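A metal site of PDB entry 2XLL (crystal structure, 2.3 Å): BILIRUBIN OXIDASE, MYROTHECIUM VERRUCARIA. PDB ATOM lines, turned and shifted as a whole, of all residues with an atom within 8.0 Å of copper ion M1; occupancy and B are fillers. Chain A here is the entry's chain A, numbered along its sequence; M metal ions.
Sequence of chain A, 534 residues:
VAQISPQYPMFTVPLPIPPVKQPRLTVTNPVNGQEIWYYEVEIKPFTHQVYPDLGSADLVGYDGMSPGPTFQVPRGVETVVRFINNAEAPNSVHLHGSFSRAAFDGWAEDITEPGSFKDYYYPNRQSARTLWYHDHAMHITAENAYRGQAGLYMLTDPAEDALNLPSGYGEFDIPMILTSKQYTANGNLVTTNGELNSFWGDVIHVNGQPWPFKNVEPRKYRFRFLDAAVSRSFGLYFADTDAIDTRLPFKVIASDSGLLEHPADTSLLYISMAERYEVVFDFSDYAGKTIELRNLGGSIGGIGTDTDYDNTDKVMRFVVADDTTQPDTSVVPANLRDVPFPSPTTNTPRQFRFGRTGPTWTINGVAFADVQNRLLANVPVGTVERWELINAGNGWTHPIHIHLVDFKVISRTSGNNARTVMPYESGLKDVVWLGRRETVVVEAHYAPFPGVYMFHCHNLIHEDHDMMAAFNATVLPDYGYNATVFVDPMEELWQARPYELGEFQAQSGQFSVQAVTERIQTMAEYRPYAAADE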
ATOM      1  N   HIS A  94      31.336  25.675 -23.758  1.00  0.00           N
ATOM      2  CA  HIS A  94      30.258  25.418 -24.682  1.00  0.00           C
ATOM      3  C   HIS A  94      29.954  26.657 -25.484  1.00  0.00           C
ATOM      4  O   HIS A  94      29.644  27.694 -24.916  1.00  0.00           O
ATOM      5  CB  HIS A  94      28.974  25.025 -23.954  1.00  0.00           C
ATOM      6  CG  HIS A  94      27.802  24.899 -24.866  1.00  0.00           C
ATOM      7  ND1 HIS A  94      27.865  24.233 -26.066  1.00  0.00           N
ATOM      8  CD2 HIS A  94      26.551  25.402 -24.777  1.00  0.00           C
ATOM      9  CE1 HIS A  94      26.697  24.302 -26.670  1.00  0.00           C
ATOM     10  NE2 HIS A  94      25.881  25.010 -25.910  1.00  0.00           N
ATOM     11  N   HIS A  96      27.284  28.118 -27.363  1.00  0.00           N
ATOM     12  CA  HIS A  96      25.846  27.960 -27.460  1.00  0.00           C
ATOM     13  C   HIS A  96      25.280  28.606 -28.725  1.00  0.00           C
ATOM     14  O   HIS A  96      25.433  29.805 -28.937  1.00  0.00           O
ATOM     15  CB  HIS A  96      25.220  28.630 -26.238  1.00  0.00           C
ATOM     16  CG  HIS A  96      23.740  28.470 -26.134  1.00  0.00           C
ATOM     17  ND1 HIS A  96      23.120  28.119 -24.955  1.00  0.00           N
ATOM     18  CD2 HIS A  96      22.754  28.624 -27.054  1.00  0.00           C
ATOM     19  CE1 HIS A  96      21.814  28.059 -25.149  1.00  0.00           C
ATOM     20  NE2 HIS A  96      21.564  28.362 -26.412  1.00  0.00           N
ATOM     21  N   ASP A 105      31.596  20.448 -28.149  1.00  0.00           N
ATOM     22  CA  ASP A 105      30.323  21.099 -27.826  1.00  0.00           C
ATOM     23  C   ASP A 105      30.229  21.473 -26.364  1.00  0.00           C
ATOM     24  O   ASP A 105      29.281  22.120 -25.959  1.00  0.00           O
ATOM     25  CB  ASP A 105      29.135  20.194 -28.189  1.00  0.00           C
ATOM     26  CG  ASP A 105      27.804  20.943 -28.219  1.00  0.00           C
ATOM     27  OD1 ASP A 105      26.825  20.405 -27.679  1.00  0.00           O
ATOM     28  OD2 ASP A 105      27.732  22.051 -28.810  1.00  0.00           O
ATOM     29  N   GLY A 106      31.203  21.052 -25.586  1.00  0.00           N
ATOM     30  CA  GLY A 106      31.177  21.346 -24.161  1.00  0.00           C
ATOM     31  C   GLY A 106      30.395  20.344 -23.340  1.00  0.00           C
ATOM     32  O   GLY A 106      29.762  20.702 -22.353  1.00  0.00           O
ATOM     33  N   TRP A 107      30.435  19.079 -23.741  1.00  0.00           N
ATOM     34  CA  TRP A 107      29.789  18.032 -22.970  1.00  0.00           C
ATOM     35  C   TRP A 107      30.200  18.200 -21.512  1.00  0.00           C
ATOM     36  O   TRP A 107      31.376  18.415 -21.203  1.00  0.00           O
ATOM     37  CB  TRP A 107      30.226  16.669 -23.508  1.00  0.00           C
ATOM     38  CG  TRP A 107      29.820  15.457 -22.721  1.00  0.00           C
ATOM     39  CD1 TRP A 107      30.614  14.713 -21.891  1.00  0.00           C
ATOM     40  CD2 TRP A 107      28.538  14.826 -22.706  1.00  0.00           C
ATOM     41  NE1 TRP A 107      29.902  13.659 -21.370  1.00  0.00           N
ATOM     42  CE2 TRP A 107      28.625  13.701 -21.859  1.00  0.00           C
ATOM     43  CE3 TRP A 107      27.323  15.102 -23.339  1.00  0.00           C
ATOM     44  CZ2 TRP A 107      27.536  12.860 -21.615  1.00  0.00           C
ATOM     45  CZ3 TRP A 107      26.241  14.264 -23.089  1.00  0.00           C
ATOM     46  CH2 TRP A 107      26.358  13.158 -22.238  1.00  0.00           C
ATOM     47  N   ALA A 108      29.213  18.108 -20.628  1.00  0.00           N
ATOM     48  CA  ALA A 108      29.415  18.418 -19.210  1.00  0.00           C
ATOM     49  C   ALA A 108      30.575  17.694 -18.540  1.00  0.00           C
ATOM     50  O   ALA A 108      31.213  18.246 -17.647  1.00  0.00           O
ATOM     51  CB  ALA A 108      28.121  18.187 -18.423  1.00  0.00           C
ATOM     52  N   HIS A 134      30.322  29.825 -22.957  1.00  0.00           N
ATOM     53  CA  HIS A 134      30.283  29.823 -21.504  1.00  0.00           C
ATOM     54  C   HIS A 134      30.541  28.445 -20.959  1.00  0.00           C
ATOM     55  O   HIS A 134      30.452  27.452 -21.670  1.00  0.00           O
ATOM     56  CB  HIS A 134      28.924  30.288 -21.047  1.00  0.00           C
ATOM     57  CG  HIS A 134      27.831  29.311 -21.356  1.00  0.00           C
ATOM     58  ND1 HIS A 134      27.722  28.098 -20.720  1.00  0.00           N
ATOM     59  CD2 HIS A 134      26.783  29.387 -22.218  1.00  0.00           C
ATOM     60  CE1 HIS A 134      26.657  27.456 -21.184  1.00  0.00           C
ATOM     61  NE2 HIS A 134      26.074  28.222 -22.082  1.00  0.00           N
ATOM     62  N   ASP A 135      30.838  28.383 -19.657  1.00  0.00           N
ATOM     63  CA  ASP A 135      31.214  27.132 -19.021  1.00  0.00           C
ATOM     64  C   ASP A 135      30.048  26.150 -18.906  1.00  0.00           C
ATOM     65  O   ASP A 135      28.889  26.553 -18.809  1.00  0.00           O
ATOM     66  CB  ASP A 135      31.780  27.380 -17.629  1.00  0.00           C
ATOM     67  CG  ASP A 135      32.356  26.121 -17.020  1.00  0.00           C
ATOM     68  OD1 ASP A 135      33.359  25.617 -17.567  1.00  0.00           O
ATOM     69  OD2 ASP A 135      31.799  25.632 -16.001  1.00  0.00           O
ATOM     70  N   HIS A 136      30.388  24.872 -18.853  1.00  0.00           N
ATOM     71  CA  HIS A 136      29.378  23.830 -18.773  1.00  0.00           C
ATOM     72  C   HIS A 136      29.877  22.664 -17.906  1.00  0.00           C
ATOM     73  O   HIS A 136      29.311  21.584 -17.935  1.00  0.00           O
ATOM     74  CB  HIS A 136      29.068  23.339 -20.189  1.00  0.00           C
ATOM     75  CG  HIS A 136      27.616  23.081 -20.458  1.00  0.00           C
ATOM     76  ND1 HIS A 136      26.844  22.251 -19.665  1.00  0.00           N
ATOM     77  CD2 HIS A 136      26.802  23.533 -21.439  1.00  0.00           C
ATOM     78  CE1 HIS A 136      25.614  22.223 -20.142  1.00  0.00           C
ATOM     79  NE2 HIS A 136      25.561  22.977 -21.225  1.00  0.00           N
ATOM     80  N   THR A 141      28.514  24.371 -13.065  1.00  0.00           N
ATOM     81  CA  THR A 141      28.244  25.323 -14.143  1.00  0.00           C
ATOM     82  C   THR A 141      27.723  26.662 -13.579  1.00  0.00           C
ATOM     83  O   THR A 141      28.114  27.744 -14.027  1.00  0.00           O
ATOM     84  CB  THR A 141      27.239  24.744 -15.151  1.00  0.00           C
ATOM     85  OG1 THR A 141      27.848  23.654 -15.848  1.00  0.00           O
ATOM     86  CG2 THR A 141      26.820  25.788 -16.155  1.00  0.00           C
ATOM     87  N   ALA A 274      19.676  32.169 -21.293  1.00  0.00           N
ATOM     88  CA  ALA A 274      20.317  31.681 -22.523  1.00  0.00           C
ATOM     89  C   ALA A 274      19.699  32.225 -23.807  1.00  0.00           C
ATOM     90  O   ALA A 274      20.206  32.004 -24.891  1.00  0.00           O
ATOM     91  CB  ALA A 274      20.356  30.155 -22.554  1.00  0.00           C
ATOM     92  N   HIS A 401      16.785  24.213 -23.157  1.00  0.00           N
ATOM     93  CA  HIS A 401      17.784  24.317 -24.215  1.00  0.00           C
ATOM     94  C   HIS A 401      18.156  22.967 -24.828  1.00  0.00           C
ATOM     95  O   HIS A 401      18.448  22.013 -24.130  1.00  0.00           O
ATOM     96  CB  HIS A 401      19.048  24.988 -23.686  1.00  0.00           C
ATOM     97  CG  HIS A 401      20.138  25.065 -24.691  1.00  0.00           C
ATOM     98  ND1 HIS A 401      19.949  25.568 -25.959  1.00  0.00           N
ATOM     99  CD2 HIS A 401      21.435  24.665 -24.630  1.00  0.00           C
ATOM    100  CE1 HIS A 401      21.081  25.494 -26.629  1.00  0.00           C
ATOM    101  NE2 HIS A 401      21.998  24.954 -25.858  1.00  0.00           N
ATOM    102  N   ILE A 402      18.111  22.906 -26.145  1.00  0.00           N
ATOM    103  CA  ILE A 402      18.469  21.691 -26.853  1.00  0.00           C
ATOM    104  C   ILE A 402      19.703  21.992 -27.685  1.00  0.00           C
ATOM    105  O   ILE A 402      19.670  22.901 -28.505  1.00  0.00           O
ATOM    106  CB  ILE A 402      17.348  21.254 -27.801  1.00  0.00           C
ATOM    107  CG1 ILE A 402      16.040  21.068 -27.035  1.00  0.00           C
ATOM    108  CG2 ILE A 402      17.737  19.971 -28.494  1.00  0.00           C
ATOM    109  CD1 ILE A 402      14.896  20.698 -27.926  1.00  0.00           C
ATOM    110  N   HIS A 403      20.766  21.220 -27.476  1.00  0.00           N
ATOM    111  CA  HIS A 403      22.018  21.407 -28.197  1.00  0.00           C
ATOM    112  C   HIS A 403      21.901  20.967 -29.647  1.00  0.00           C
ATOM    113  O   HIS A 403      20.940  20.309 -30.015  1.00  0.00           O
ATOM    114  CB  HIS A 403      23.135  20.620 -27.528  1.00  0.00           C
ATOM    115  CG  HIS A 403      23.728  21.300 -26.336  1.00  0.00           C
ATOM    116  ND1 HIS A 403      25.086  21.421 -26.150  1.00  0.00           N
ATOM    117  CD2 HIS A 403      23.140  21.929 -25.292  1.00  0.00           C
ATOM    118  CE1 HIS A 403      25.327  22.070 -25.026  1.00  0.00           C
ATOM    119  NE2 HIS A 403      24.154  22.394 -24.488  1.00  0.00           N
ATOM    120  N   TYR A 453      24.602  14.478 -27.494  1.00  0.00           N
ATOM    121  CA  TYR A 453      24.426  15.896 -27.187  1.00  0.00           C
ATOM    122  C   TYR A 453      23.521  16.117 -25.963  1.00  0.00           C
ATOM    123  O   TYR A 453      22.633  15.310 -25.677  1.00  0.00           O
ATOM    124  CB  TYR A 453      23.803  16.622 -28.380  1.00  0.00           C
ATOM    125  CG  TYR A 453      24.693  16.806 -29.605  1.00  0.00           C
ATOM    126  CD1 TYR A 453      25.662  17.788 -29.643  1.00  0.00           C
ATOM    127  CD2 TYR A 453      24.526  16.009 -30.725  1.00  0.00           C
ATOM    128  CE1 TYR A 453      26.451  17.981 -30.777  1.00  0.00           C
ATOM    129  CE2 TYR A 453      25.309  16.186 -31.860  1.00  0.00           C
ATOM    130  CZ  TYR A 453      26.269  17.169 -31.875  1.00  0.00           C
ATOM    131  OH  TYR A 453      27.071  17.344 -32.999  1.00  0.00           O
ATOM    132  N   MET A 454      23.732  17.230 -25.271  1.00  0.00           N
ATOM    133  CA  MET A 454      22.909  17.611 -24.134  1.00  0.00           C
ATOM    134  C   MET A 454      21.639  18.357 -24.492  1.00  0.00           C
ATOM    135  O   MET A 454      21.517  19.000 -25.557  1.00  0.00           O
ATOM    136  CB  MET A 454      23.703  18.428 -23.116  1.00  0.00           C
ATOM    137  CG  MET A 454      24.851  17.659 -22.443  1.00  0.00           C
ATOM    138  SD  MET A 454      25.894  18.673 -21.368  1.00  0.00           S
ATOM    139  CE  MET A 454      26.491  19.868 -22.574  1.00  0.00           C
ATOM    140  N   PHE A 455      20.679  18.240 -23.580  1.00  0.00           N
ATOM    141  CA  PHE A 455      19.541  19.155 -23.526  1.00  0.00           C
ATOM    142  C   PHE A 455      19.110  19.308 -22.059  1.00  0.00           C
ATOM    143  O   PHE A 455      19.260  18.374 -21.276  1.00  0.00           O
ATOM    144  CB  PHE A 455      18.407  18.703 -24.452  1.00  0.00           C
ATOM    145  CG  PHE A 455      17.541  17.615 -23.903  1.00  0.00           C
ATOM    146  CD1 PHE A 455      17.887  16.293 -24.052  1.00  0.00           C
ATOM    147  CD2 PHE A 455      16.352  17.909 -23.288  1.00  0.00           C
ATOM    148  CE1 PHE A 455      17.070  15.303 -23.571  1.00  0.00           C
ATOM    149  CE2 PHE A 455      15.542  16.921 -22.800  1.00  0.00           C
ATOM    150  CZ  PHE A 455      15.901  15.618 -22.941  1.00  0.00           C
ATOM    151  N   HIS A 456      18.626  20.469 -21.669  1.00  0.00           N
ATOM    152  CA  HIS A 456      18.455  20.764 -20.241  1.00  0.00           C
ATOM    153  C   HIS A 456      17.722  22.073 -20.022  1.00  0.00           C
ATOM    154  O   HIS A 456      17.464  22.818 -20.970  1.00  0.00           O
ATOM    155  CB  HIS A 456      19.829  20.857 -19.548  1.00  0.00           C
ATOM    156  CG  HIS A 456      20.739  21.870 -20.173  1.00  0.00           C
ATOM    157  ND1 HIS A 456      20.886  23.146 -19.672  1.00  0.00           N
ATOM    158  CD2 HIS A 456      21.522  21.808 -21.275  1.00  0.00           C
ATOM    159  CE1 HIS A 456      21.749  23.820 -20.428  1.00  0.00           C
ATOM    160  NE2 HIS A 456      22.146  23.025 -21.404  1.00  0.00           N
ATOM    161  N   CYS A 457      17.391  22.369 -18.776  1.00  0.00           N
ATOM    162  CA  CYS A 457      16.942  23.692 -18.407  1.00  0.00           C
ATOM    163  C   CYS A 457      18.168  24.599 -18.303  1.00  0.00           C
ATOM    164  O   CYS A 457      19.220  24.177 -17.857  1.00  0.00           O
ATOM    165  CB  CYS A 457      16.222  23.650 -17.062  1.00  0.00           C
ATOM    166  SG  CYS A 457      15.695  25.291 -16.507  1.00  0.00           S
ATOM    167  N   HIS A 458      18.025  25.863 -18.673  1.00  0.00           N
ATOM    168  CA  HIS A 458      19.177  26.751 -18.589  1.00  0.00           C
ATOM    169  C   HIS A 458      19.164  27.642 -17.331  1.00  0.00           C
ATOM    170  O   HIS A 458      19.980  28.566 -17.192  1.00  0.00           O
ATOM    171  CB  HIS A 458      19.327  27.587 -19.869  1.00  0.00           C
ATOM    172  CG  HIS A 458      20.753  27.778 -20.285  1.00  0.00           C
ATOM    173  ND1 HIS A 458      21.612  28.624 -19.614  1.00  0.00           N
ATOM    174  CD2 HIS A 458      21.468  27.219 -21.283  1.00  0.00           C
ATOM    175  CE1 HIS A 458      22.801  28.590 -20.195  1.00  0.00           C
ATOM    176  NE2 HIS A 458      22.739  27.749 -21.209  1.00  0.00           N
ATOM    177  N   LEU A 460      20.720  27.731 -14.340  1.00  0.00           N
ATOM    178  CA  LEU A 460      21.936  27.029 -13.959  1.00  0.00           C
ATOM    179  C   LEU A 460      21.830  26.273 -12.640  1.00  0.00           C
ATOM    180  O   LEU A 460      22.442  25.228 -12.464  1.00  0.00           O
ATOM    181  CB  LEU A 460      23.121  27.989 -13.928  1.00  0.00           C
ATOM    182  CG  LEU A 460      23.315  28.783 -15.221  1.00  0.00           C
ATOM    183  CD1 LEU A 460      24.661  29.454 -15.278  1.00  0.00           C
ATOM    184  CD2 LEU A 460      23.153  27.870 -16.402  1.00  0.00           C
ATOM    185  N   GLU A 463      19.933  23.242 -13.567  1.00  0.00           N
ATOM    186  CA  GLU A 463      20.841  22.478 -14.401  1.00  0.00           C
ATOM    187  C   GLU A 463      21.815  21.656 -13.576  1.00  0.00           C
ATOM    188  O   GLU A 463      22.016  20.473 -13.834  1.00  0.00           O
ATOM    189  CB  GLU A 463      21.596  23.406 -15.344  1.00  0.00           C
ATOM    190  CG  GLU A 463      22.363  22.717 -16.462  1.00  0.00           C
ATOM    191  CD  GLU A 463      23.154  23.704 -17.302  1.00  0.00           C
ATOM    192  OE1 GLU A 463      22.565  24.742 -17.685  1.00  0.00           O
ATOM    193  OE2 GLU A 463      24.349  23.471 -17.548  1.00  0.00           O
ATOM    194  N   MET A 468      19.333  17.898 -16.333  1.00  0.00           N
ATOM    195  CA  MET A 468      20.049  17.804 -17.580  1.00  0.00           C
ATOM    196  C   MET A 468      19.991  16.359 -18.054  1.00  0.00           C
ATOM    197  O   MET A 468      19.970  15.442 -17.248  1.00  0.00           O
ATOM    198  CB  MET A 468      21.493  18.257 -17.379  1.00  0.00           C
ATOM    199  CG  MET A 468      22.352  18.268 -18.628  1.00  0.00           C
ATOM    200  SD  MET A 468      23.731  19.460 -18.483  1.00  0.00           S
ATOM    201  CE  MET A 468      24.697  18.691 -17.194  1.00  0.00           C
ATOM    202  N   ALA A 469      19.921  16.183 -19.368  1.00  0.00           N
ATOM    203  CA  ALA A 469      19.883  14.858 -19.980  1.00  0.00           C
ATOM    204  C   ALA A 469      20.557  14.864 -21.351  1.00  0.00           C
ATOM    205  O   ALA A 469      21.116  15.891 -21.770  1.00  0.00           O
ATOM    206  CB  ALA A 469      18.450  14.363 -20.081  1.00  0.00           C
HETATM  207 CU    CU M   1      23.881  23.084 -22.606  1.00  0.00          CU
HETATM  208 CU    CU M   2      23.921  25.243 -26.055  1.00  0.00          CU
HETATM  209 CU    CU M   3      24.097  27.930 -23.019  1.00  0.00          CU
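The backbone carbonyl oxygen (O) of His 136 lies close to the side-chain hydroxyl (OG1) of Thr 141, at 3.3 Å. NE2 of His 96 lies close to ND1 of His 401, at 3.3 Å. OD1 of Asp 105 lies within hydrogen-bond range of ND1 of His 403 (2.5 Å). The backbone NH (N) of His 403 sits close to the backbone carbonyl oxygen (O) of Met 454 (3.0 Å). N of His 401 is in hydrogen-bond range of O of His 456 (2.7 Å). ND1 of His 456 lies close to OE1 of Glu 463, 3.1 Å away. A ring nitrogen (ND1) of His 136 lies close to the side-chain carboxylate of Glu 463 (3.5 Å).
Residues that only touch copper ion M1: His 401. Within 4 Å of copper ion M1: His 136, His 401, His 403 and His 456. The nearest printed residue that does not touch copper ion M1 is Met 454 (4.1 Å).
Copper ion M1 is bound by a ring nitrogen (NE2) of His 403 (2.0 Å), a ring nitrogen (NE2) of His 456 (2.1 Å) and a ring nitrogen (NE2) of His 136 (2.2 Å). Copper ion M1 has three donor atoms within binding distance.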
